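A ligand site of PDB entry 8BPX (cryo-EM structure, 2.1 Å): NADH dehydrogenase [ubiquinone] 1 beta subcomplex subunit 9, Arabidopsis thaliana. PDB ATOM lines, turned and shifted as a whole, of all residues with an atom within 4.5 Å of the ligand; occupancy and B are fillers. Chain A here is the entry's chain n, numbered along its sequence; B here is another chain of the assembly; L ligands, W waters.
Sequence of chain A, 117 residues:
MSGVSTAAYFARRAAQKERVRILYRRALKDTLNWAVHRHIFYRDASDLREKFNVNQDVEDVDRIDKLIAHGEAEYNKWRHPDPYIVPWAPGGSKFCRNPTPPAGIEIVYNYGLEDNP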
ATOM      1  N   ARG A  13     -16.360  18.813 -23.924  1.00  0.00           N
ATOM      2  CA  ARG A  13     -14.925  19.051 -24.168  1.00  0.00           C
ATOM      3  C   ARG A  13     -14.769  20.464 -24.729  1.00  0.00           C
ATOM      4  O   ARG A  13     -13.827  21.189 -24.305  1.00  0.00           O
ATOM      5  CB  ARG A  13     -14.354  17.898 -25.019  1.00  0.00           C
ATOM      6  CG  ARG A  13     -14.107  16.617 -24.250  1.00  0.00           C
ATOM      7  CD  ARG A  13     -12.814  16.547 -23.473  1.00  0.00           C
ATOM      8  NE  ARG A  13     -11.662  17.011 -24.235  1.00  0.00           N
ATOM      9  CZ  ARG A  13     -11.042  18.156 -24.013  1.00  0.00           C
ATOM     10  NH1 ARG A  13     -11.471  18.967 -23.063  1.00  0.00           N
ATOM     11  NH2 ARG A  13     -10.001  18.492 -24.744  1.00  0.00           N
ATOM     12  N   LYS A  17     -12.585  23.666 -23.238  1.00  0.00           N
ATOM     13  CA  LYS A  17     -11.658  24.439 -24.081  1.00  0.00           C
ATOM     14  C   LYS A  17     -11.868  25.932 -23.856  1.00  0.00           C
ATOM     15  O   LYS A  17     -10.867  26.610 -23.702  1.00  0.00           O
ATOM     16  CB  LYS A  17     -11.857  23.960 -25.501  1.00  0.00           C
ATOM     17  CG  LYS A  17     -11.231  22.623 -25.857  1.00  0.00           C
ATOM     18  CD  LYS A  17     -11.345  22.336 -27.328  1.00  0.00           C
ATOM     19  CE  LYS A  17     -10.991  20.915 -27.691  1.00  0.00           C
ATOM     20  NZ  LYS A  17     -11.563  19.962 -26.711  1.00  0.00           N
ATOM     21  N   VAL A  20     -10.310  27.022 -20.601  1.00  0.00           N
ATOM     22  CA  VAL A  20      -8.829  27.093 -20.681  1.00  0.00           C
ATOM     23  C   VAL A  20      -8.407  28.351 -21.491  1.00  0.00           C
ATOM     24  O   VAL A  20      -7.619  29.082 -20.959  1.00  0.00           O
ATOM     25  CB  VAL A  20      -8.167  25.791 -21.151  1.00  0.00           C
ATOM     26  CG1 VAL A  20      -6.658  25.900 -21.275  1.00  0.00           C
ATOM     27  CG2 VAL A  20      -8.562  24.620 -20.280  1.00  0.00           C
ATOM     28  N   ARG A  21      -9.013  28.606 -22.643  1.00  0.00           N
ATOM     29  CA  ARG A  21      -8.686  29.784 -23.490  1.00  0.00           C
ATOM     30  C   ARG A  21      -8.956  31.115 -22.760  1.00  0.00           C
ATOM     31  O   ARG A  21      -8.199  32.040 -22.952  1.00  0.00           O
ATOM     32  CB  ARG A  21      -9.373  29.669 -24.846  1.00  0.00           C
ATOM     33  CG  ARG A  21      -8.767  28.622 -25.764  1.00  0.00           C
ATOM     34  CD  ARG A  21      -9.248  28.776 -27.190  1.00  0.00           C
ATOM     35  NE  ARG A  21     -10.683  28.969 -27.208  1.00  0.00           N
ATOM     36  CZ  ARG A  21     -11.576  28.006 -27.337  1.00  0.00           C
ATOM     37  NH1 ARG A  21     -11.195  26.755 -27.520  1.00  0.00           N
ATOM     38  NH2 ARG A  21     -12.856  28.305 -27.287  1.00  0.00           N
ATOM     39  N   LEU A  23      -9.055  31.417 -19.355  1.00  0.00           N
ATOM     40  CA  LEU A  23      -8.094  31.422 -18.213  1.00  0.00           C
ATOM     41  C   LEU A  23      -6.743  31.930 -18.726  1.00  0.00           C
ATOM     42  O   LEU A  23      -6.157  32.815 -18.067  1.00  0.00           O
ATOM     43  CB  LEU A  23      -7.969  30.037 -17.589  1.00  0.00           C
ATOM     44  CG  LEU A  23      -6.872  29.888 -16.527  1.00  0.00           C
ATOM     45  CD1 LEU A  23      -7.179  30.723 -15.289  1.00  0.00           C
ATOM     46  CD2 LEU A  23      -6.646  28.442 -16.148  1.00  0.00           C
ATOM     47  N   ALA A  27      -4.713  35.307 -17.416  1.00  0.00           N
ATOM     48  CA  ALA A  27      -3.376  35.090 -16.796  1.00  0.00           C
ATOM     49  C   ALA A  27      -2.346  35.927 -17.564  1.00  0.00           C
ATOM     50  O   ALA A  27      -1.625  36.662 -16.903  1.00  0.00           O
ATOM     51  CB  ALA A  27      -3.010  33.608 -16.712  1.00  0.00           C
ATOM     52  N   ASP A  30      -2.703  39.688 -16.855  1.00  0.00           N
ATOM     53  CA  ASP A  30      -2.233  39.958 -15.502  1.00  0.00           C
ATOM     54  C   ASP A  30      -0.709  39.885 -15.404  1.00  0.00           C
ATOM     55  O   ASP A  30      -0.188  40.534 -14.562  1.00  0.00           O
ATOM     56  CB  ASP A  30      -2.938  39.032 -14.519  1.00  0.00           C
ATOM     57  CG  ASP A  30      -3.113  39.645 -13.158  1.00  0.00           C
ATOM     58  OD1 ASP A  30      -3.866  40.623 -13.061  1.00  0.00           O
ATOM     59  OD2 ASP A  30      -2.486  39.145 -12.210  1.00  0.00           O
ATOM     60  N   LEU A  48       4.450  31.382 -18.500  1.00  0.00           N
ATOM     61  CA  LEU A  48       3.015  31.031 -18.316  1.00  0.00           C
ATOM     62  C   LEU A  48       2.559  30.085 -19.435  1.00  0.00           C
ATOM     63  O   LEU A  48       1.815  29.014 -19.177  1.00  0.00           O
ATOM     64  CB  LEU A  48       2.211  32.324 -18.247  1.00  0.00           C
ATOM     65  CG  LEU A  48       0.700  32.192 -18.203  1.00  0.00           C
ATOM     66  CD1 LEU A  48       0.220  31.904 -16.786  1.00  0.00           C
ATOM     67  CD2 LEU A  48       0.062  33.443 -18.747  1.00  0.00           C
ATOM     68  N   LYS A  51       3.641  26.562 -18.564  1.00  0.00           N
ATOM     69  CA  LYS A  51       2.657  25.866 -17.699  1.00  0.00           C
ATOM     70  C   LYS A  51       1.474  25.234 -18.529  1.00  0.00           C
ATOM     71  O   LYS A  51       1.183  23.849 -18.628  1.00  0.00           O
ATOM     72  CB  LYS A  51       2.230  26.864 -16.620  1.00  0.00           C
ATOM     73  CG  LYS A  51       3.298  27.400 -15.693  1.00  0.00           C
ATOM     74  CD  LYS A  51       2.729  28.307 -14.641  1.00  0.00           C
ATOM     75  CE  LYS A  51       3.786  29.048 -13.865  1.00  0.00           C
ATOM     76  NZ  LYS A  51       3.269  29.600 -12.587  1.00  0.00           N
ATOM     77  N   PHE A  52       0.863  26.106 -19.332  1.00  0.00           N
ATOM     78  CA  PHE A  52      -0.260  25.465 -20.082  1.00  0.00           C
ATOM     79  C   PHE A  52       0.270  24.369 -21.019  1.00  0.00           C
ATOM     80  O   PHE A  52      -0.341  23.335 -21.179  1.00  0.00           O
ATOM     81  CB  PHE A  52      -1.121  26.491 -20.812  1.00  0.00           C
ATOM     82  CG  PHE A  52      -1.935  27.434 -19.953  1.00  0.00           C
ATOM     83  CD1 PHE A  52      -1.332  28.431 -19.220  1.00  0.00           C
ATOM     84  CD2 PHE A  52      -3.313  27.336 -19.916  1.00  0.00           C
ATOM     85  CE1 PHE A  52      -2.080  29.305 -18.446  1.00  0.00           C
ATOM     86  CE2 PHE A  52      -4.061  28.210 -19.142  1.00  0.00           C
ATOM     87  CZ  PHE A  52      -3.443  29.185 -18.400  1.00  0.00           C
ATOM     88  N   ASN A  55       0.630  20.804 -19.570  1.00  0.00           N
ATOM     89  CA  ASN A  55      -0.607  19.949 -19.576  1.00  0.00           C
ATOM     90  C   ASN A  55      -1.400  19.904 -20.889  1.00  0.00           C
ATOM     91  O   ASN A  55      -2.464  19.256 -20.875  1.00  0.00           O
ATOM     92  CB  ASN A  55      -1.659  20.340 -18.531  1.00  0.00           C
ATOM     93  CG  ASN A  55      -1.121  20.377 -17.133  1.00  0.00           C
ATOM     94  OD1 ASN A  55      -0.756  21.442 -16.641  1.00  0.00           O
ATOM     95  ND2 ASN A  55      -1.093  19.242 -16.480  1.00  0.00           N
ATOM     96  N   GLN A  56      -0.951  20.520 -21.984  1.00  0.00           N
ATOM     97  CA  GLN A  56      -1.753  20.616 -23.267  1.00  0.00           C
ATOM     98  C   GLN A  56      -2.229  19.275 -23.810  1.00  0.00           C
ATOM     99  O   GLN A  56      -3.160  19.209 -24.605  1.00  0.00           O
ATOM    100  CB  GLN A  56      -0.952  21.215 -24.429  1.00  0.00           C
ATOM    101  CG  GLN A  56       0.194  20.377 -24.954  1.00  0.00           C
ATOM    102  CD  GLN A  56       1.068  21.162 -25.907  1.00  0.00           C
ATOM    103  OE1 GLN A  56       1.345  22.350 -25.706  1.00  0.00           O
ATOM    104  NE2 GLN A  56       1.517  20.506 -26.960  1.00  0.00           N
ATOM    105  N   VAL A  58      -3.136  16.400 -22.119  1.00  0.00           N
ATOM    106  CA  VAL A  58      -3.993  15.491 -21.335  1.00  0.00           C
ATOM    107  C   VAL A  58      -5.306  15.159 -22.062  1.00  0.00           C
ATOM    108  O   VAL A  58      -5.878  16.018 -22.715  1.00  0.00           O
ATOM    109  CB  VAL A  58      -4.171  16.065 -19.903  1.00  0.00           C
ATOM    110  CG1 VAL A  58      -5.302  15.414 -19.127  1.00  0.00           C
ATOM    111  CG2 VAL A  58      -2.886  16.175 -19.114  1.00  0.00           C
ATOM    112  N   ILE A  64      -9.031  17.087 -16.495  1.00  0.00           N
ATOM    113  CA  ILE A  64      -9.064  18.420 -17.139  1.00  0.00           C
ATOM    114  C   ILE A  64      -9.882  19.312 -16.218  1.00  0.00           C
ATOM    115  O   ILE A  64      -9.419  20.415 -15.942  1.00  0.00           O
ATOM    116  CB  ILE A  64      -9.555  18.424 -18.608  1.00  0.00           C
ATOM    117  CG1 ILE A  64      -8.574  17.722 -19.561  1.00  0.00           C
ATOM    118  CG2 ILE A  64      -9.888  19.824 -19.078  1.00  0.00           C
ATOM    119  CD1 ILE A  64      -9.227  17.262 -20.845  1.00  0.00           C
ATOM    120  N   LEU A  67      -7.836  20.329 -13.205  1.00  0.00           N
ATOM    121  CA  LEU A  67      -6.804  21.323 -13.596  1.00  0.00           C
ATOM    122  C   LEU A  67      -7.424  22.685 -13.886  1.00  0.00           C
ATOM    123  O   LEU A  67      -6.826  23.683 -13.585  1.00  0.00           O
ATOM    124  CB  LEU A  67      -6.012  20.791 -14.801  1.00  0.00           C
ATOM    125  CG  LEU A  67      -5.171  19.530 -14.573  1.00  0.00           C
ATOM    126  CD1 LEU A  67      -4.561  19.020 -15.859  1.00  0.00           C
ATOM    127  CD2 LEU A  67      -4.103  19.797 -13.524  1.00  0.00           C
ATOM    128  N   ILE A  68      -8.584  22.710 -14.526  1.00  0.00           N
ATOM    129  CA  ILE A  68      -9.223  23.987 -14.792  1.00  0.00           C
ATOM    130  C   ILE A  68      -9.581  24.680 -13.483  1.00  0.00           C
ATOM    131  O   ILE A  68      -9.312  25.867 -13.294  1.00  0.00           O
ATOM    132  CB  ILE A  68     -10.467  23.821 -15.685  1.00  0.00           C
ATOM    133  CG1 ILE A  68     -10.061  23.440 -17.113  1.00  0.00           C
ATOM    134  CG2 ILE A  68     -11.278  25.088 -15.717  1.00  0.00           C
ATOM    135  CD1 ILE A  68     -11.222  22.948 -17.946  1.00  0.00           C
ATOM    136  N   GLY A  71      -6.451  25.990 -11.833  1.00  0.00           N
ATOM    137  CA  GLY A  71      -5.958  27.165 -12.565  1.00  0.00           C
ATOM    138  C   GLY A  71      -6.781  28.407 -12.269  1.00  0.00           C
ATOM    139  O   GLY A  71      -6.153  29.434 -11.946  1.00  0.00           O
ATOM    140  N   GLU A  74      -5.918  29.554  -8.745  1.00  0.00           N
ATOM    141  CA  GLU A  74      -4.582  30.194  -8.795  1.00  0.00           C
ATOM    142  C   GLU A  74      -4.705  31.615  -9.332  1.00  0.00           C
ATOM    143  O   GLU A  74      -4.352  32.503  -8.553  1.00  0.00           O
ATOM    144  CB  GLU A  74      -3.670  29.233  -9.530  1.00  0.00           C
ATOM    145  CG  GLU A  74      -3.462  27.924  -8.785  1.00  0.00           C
ATOM    146  CD  GLU A  74      -2.885  28.065  -7.399  1.00  0.00           C
ATOM    147  OE1 GLU A  74      -1.983  28.900  -7.220  1.00  0.00           O
ATOM    148  OE2 GLU A  74      -3.333  27.324  -6.487  1.00  0.00           O
ATOM    149  N   TYR A  75      -5.338  31.850 -10.508  1.00  0.00           N
ATOM    150  CA  TYR A  75      -5.606  33.189 -11.022  1.00  0.00           C
ATOM    151  C   TYR A  75      -6.262  34.044  -9.948  1.00  0.00           C
ATOM    152  O   TYR A  75      -5.696  35.078  -9.589  1.00  0.00           O
ATOM    153  CB  TYR A  75      -6.485  33.231 -12.280  1.00  0.00           C
ATOM    154  CG  TYR A  75      -6.883  34.601 -12.759  1.00  0.00           C
ATOM    155  CD1 TYR A  75      -5.994  35.395 -13.458  1.00  0.00           C
ATOM    156  CD2 TYR A  75      -8.154  35.082 -12.535  1.00  0.00           C
ATOM    157  CE1 TYR A  75      -6.345  36.659 -13.902  1.00  0.00           C
ATOM    158  CE2 TYR A  75      -8.538  36.342 -12.976  1.00  0.00           C
ATOM    159  CZ  TYR A  75      -7.634  37.126 -13.659  1.00  0.00           C
ATOM    160  OH  TYR A  75      -8.003  38.354 -14.089  1.00  0.00           O
ATOM    161  N   TRP A  78      -3.584  34.971  -7.107  1.00  0.00           N
ATOM    162  CA  TRP A  78      -2.355  35.748  -7.454  1.00  0.00           C
ATOM    163  C   TRP A  78      -2.696  36.911  -8.359  1.00  0.00           C
ATOM    164  O   TRP A  78      -1.785  37.578  -8.867  1.00  0.00           O
ATOM    165  CB  TRP A  78      -1.286  34.777  -8.001  1.00  0.00           C
ATOM    166  CG  TRP A  78      -0.877  33.686  -7.075  1.00  0.00           C
ATOM    167  CD1 TRP A  78      -1.163  32.357  -7.206  1.00  0.00           C
ATOM    168  CD2 TRP A  78      -0.105  33.811  -5.869  1.00  0.00           C
ATOM    169  NE1 TRP A  78      -0.611  31.659  -6.171  1.00  0.00           N
ATOM    170  CE2 TRP A  78       0.038  32.509  -5.341  1.00  0.00           C
ATOM    171  CE3 TRP A  78       0.482  34.873  -5.195  1.00  0.00           C
ATOM    172  CZ2 TRP A  78       0.752  32.258  -4.163  1.00  0.00           C
ATOM    173  CZ3 TRP A  78       1.182  34.621  -4.041  1.00  0.00           C
ATOM    174  CH2 TRP A  78       1.300  33.331  -3.533  1.00  0.00           C
ATOM    175  N   GLN B  72      -6.556  28.175 -36.994  1.00  0.00           N
ATOM    176  CA  GLN B  72      -6.315  26.761 -36.650  1.00  0.00           C
ATOM    177  C   GLN B  72      -6.634  25.878 -37.853  1.00  0.00           C
ATOM    178  O   GLN B  72      -6.712  24.672 -37.686  1.00  0.00           O
ATOM    179  CB  GLN B  72      -7.147  26.332 -35.437  1.00  0.00           C
ATOM    180  CG  GLN B  72      -6.748  26.893 -34.091  1.00  0.00           C
ATOM    181  CD  GLN B  72      -7.164  25.951 -32.990  1.00  0.00           C
ATOM    182  OE1 GLN B  72      -8.205  26.113 -32.367  1.00  0.00           O
ATOM    183  NE2 GLN B  72      -6.346  24.936 -32.737  1.00  0.00           N
ATOM    184  N   ASP B  78      -2.162  26.448 -32.723  1.00  0.00           N
ATOM    185  CA  ASP B  78      -3.021  26.102 -31.597  1.00  0.00           C
ATOM    186  C   ASP B  78      -3.839  27.322 -31.179  1.00  0.00           C
ATOM    187  O   ASP B  78      -3.543  28.460 -31.562  1.00  0.00           O
ATOM    188  CB  ASP B  78      -2.174  25.586 -30.434  1.00  0.00           C
ATOM    189  CG  ASP B  78      -1.073  24.655 -30.887  1.00  0.00           C
ATOM    190  OD1 ASP B  78      -1.217  24.047 -31.970  1.00  0.00           O
ATOM    191  OD2 ASP B  78      -0.058  24.518 -30.164  1.00  0.00           O
ATOM    192  N   SER B  79      -4.929  27.027 -30.511  1.00  0.00           N
ATOM    193  CA  SER B  79      -5.845  28.099 -30.044  1.00  0.00           C
ATOM    194  C   SER B  79      -5.261  28.990 -28.923  1.00  0.00           C
ATOM    195  O   SER B  79      -5.827  30.053 -28.777  1.00  0.00           O
ATOM    196  CB  SER B  79      -7.135  27.507 -29.719  1.00  0.00           C
ATOM    197  OG  SER B  79      -7.133  27.082 -28.374  1.00  0.00           O
HETATM  198  O1  LIG L   1      -3.633  22.888 -17.139  1.00  0.00           O
HETATM  199  C1  LIG L   1      -1.554  35.169 -11.941  1.00  0.00           C
HETATM  200  O2  LIG L   1      -6.660  24.765 -29.262  1.00  0.00           O
HETATM  201  C2  LIG L   1      -2.389  34.013 -12.414  1.00  0.00           C
HETATM  202  C3  LIG L   1      -1.824  32.677 -12.028  1.00  0.00           C
HETATM  203  C4  LIG L   1      -1.477  31.814 -13.198  1.00  0.00           C
HETATM  204  O3  LIG L   1      -9.027  25.353 -28.627  1.00  0.00           O
HETATM  205  C5  LIG L   1      -2.516  30.790 -13.549  1.00  0.00           C
HETATM  206  C6  LIG L   1      -1.970  29.415 -13.790  1.00  0.00           C
HETATM  207  C7  LIG L   1      -2.868  28.549 -14.636  1.00  0.00           C
HETATM  208  C8  LIG L   1      -2.500  27.102 -14.653  1.00  0.00           C
HETATM  209  C9  LIG L   1      -1.802  26.672 -15.914  1.00  0.00           C
HETATM  210  C10 LIG L   1      -2.277  25.357 -16.484  1.00  0.00           C
HETATM  211  C11 LIG L   1      -3.771  25.199 -16.514  1.00  0.00           C
HETATM  212  C12 LIG L   1      -4.244  23.930 -17.179  1.00  0.00           C
HETATM  213  C13 LIG L   1      -6.201  24.194 -26.477  1.00  0.00           C
HETATM  214  C14 LIG L   1      -6.232  23.231 -25.298  1.00  0.00           C
HETATM  215  C15 LIG L   1      -4.883  23.225 -24.574  1.00  0.00           C
HETATM  216  C16 LIG L   1      -7.310  23.700 -24.308  1.00  0.00           C
HETATM  217  C17 LIG L   1      -6.547  21.826 -25.851  1.00  0.00           C
HETATM  218  C18 LIG L   1      -7.404  20.897 -25.000  1.00  0.00           C
HETATM  219  C19 LIG L   1      -5.778  19.906 -23.425  1.00  0.00           C
HETATM  220  C20 LIG L   1      -6.233  19.469 -22.064  1.00  0.00           C
HETATM  221  C21 LIG L   1      -6.582  20.742 -21.342  1.00  0.00           C
HETATM  222  C22 LIG L   1      -5.172  21.734 -19.523  1.00  0.00           C
HETATM  223  C23 LIG L   1      -6.184  22.521 -18.712  1.00  0.00           C
HETATM  224  N1  LIG L   1      -6.841  19.853 -24.414  1.00  0.00           N
HETATM  225  N2  LIG L   1      -5.563  21.505 -20.907  1.00  0.00           N
HETATM  226  O4  LIG L   1      -7.561  24.356 -26.965  1.00  0.00           O
HETATM  227  O5  LIG L   1      -5.317  21.195 -26.158  1.00  0.00           O
HETATM  228  O6  LIG L   1      -8.611  21.062 -24.987  1.00  0.00           O
HETATM  229  O7  LIG L   1      -7.756  21.092 -21.234  1.00  0.00           O
HETATM  230  P1  LIG L   1      -7.897  24.352 -28.542  1.00  0.00           P
HETATM  231  S1  LIG L   1      -5.797  24.141 -17.966  1.00  0.00           S
HETATM  232  O8  LIG L   1      -8.328  22.944 -28.944  1.00  0.00           O
HETATM  233  O   HOH W   1      -4.915  23.066 -28.936  1.00  0.00           O
HETATM  234  O   HOH W   2      -9.850  21.220 -22.833  1.00  0.00           O
HETATM  235  O   HOH W   3      -3.832  25.954 -27.945  1.00  0.00           O
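Water W2 bridges an oxygen (O6) of the ligand (2.5 Å) and the guanidinium group (NH1) of Arg 13 (2.8 Å).
Water W3 lies within hydrogen-bond range of the backbone NH of Ser 79 of chain B (3.0 Å) and an oxygen (O2) of the ligand (3.3 Å).
The backbone NH (N) of Ser 79 of chain B sits close to an oxygen (O2) of the ligand (3.1 Å).
OG of Ser 79 of chain B sits at hydrogen-bond distance from O2 of the ligand (2.5 Å).
NH1 of Arg 21 is in salt-bridge range of O3 of the ligand (2.8 Å).
The guanidinium group (NH2) of Arg 13 is in hydrogen-bond range of an oxygen (O6) of the ligand (2.9 Å).
The backbone carbonyl oxygen (O) of Gln 56 sits close to an oxygen (O5) of the ligand.
An oxygen (O1) of the ligand lies close to the side-chain amide oxygen of Asn 55 (3.3 Å).
The side-chain amide nitrogen (NE2) of Gln 72 of chain B sits at hydrogen-bond distance from an oxygen (O2) of the ligand.
The backbone NH of Ser 79 of chain B sits close to the side-chain amide nitrogen of Gln 72 of chain B, 3.4 Å away.
NE1 of Trp 78 of chain A is in hydrogen-bond range of OE1 of Glu 74, 3.3 Å away.
Residues that only touch the ligand: Lys 17 (3.2 Å), Ile 64 (3.3 Å), Val 58 (3.5 Å), Val 20 (3.5 Å), Tyr 75 (3.6 Å), Phe 52 (3.7 Å), Trp 78 of chain A (3.9 Å), Leu 67 (3.9 Å), Gly 71 (3.97 Å) and Leu 48 (3.97 Å).
Within 4 Å of the ligand: Arg 13, Lys 17, Val 20, Arg 21, Leu 48, Phe 52, Asn 55, Gln 56, Val 58, Ile 64, Leu 67, Gly 71, Tyr 75, Trp 78 of chain A, Gln 72 of chain B and Ser 79 of chain B.
Along chain A the residues within 4 Å of the ligand span positions 13 to 78.
The nearest printed residue that does not touch the ligand is Leu 23 (4.1 Å).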
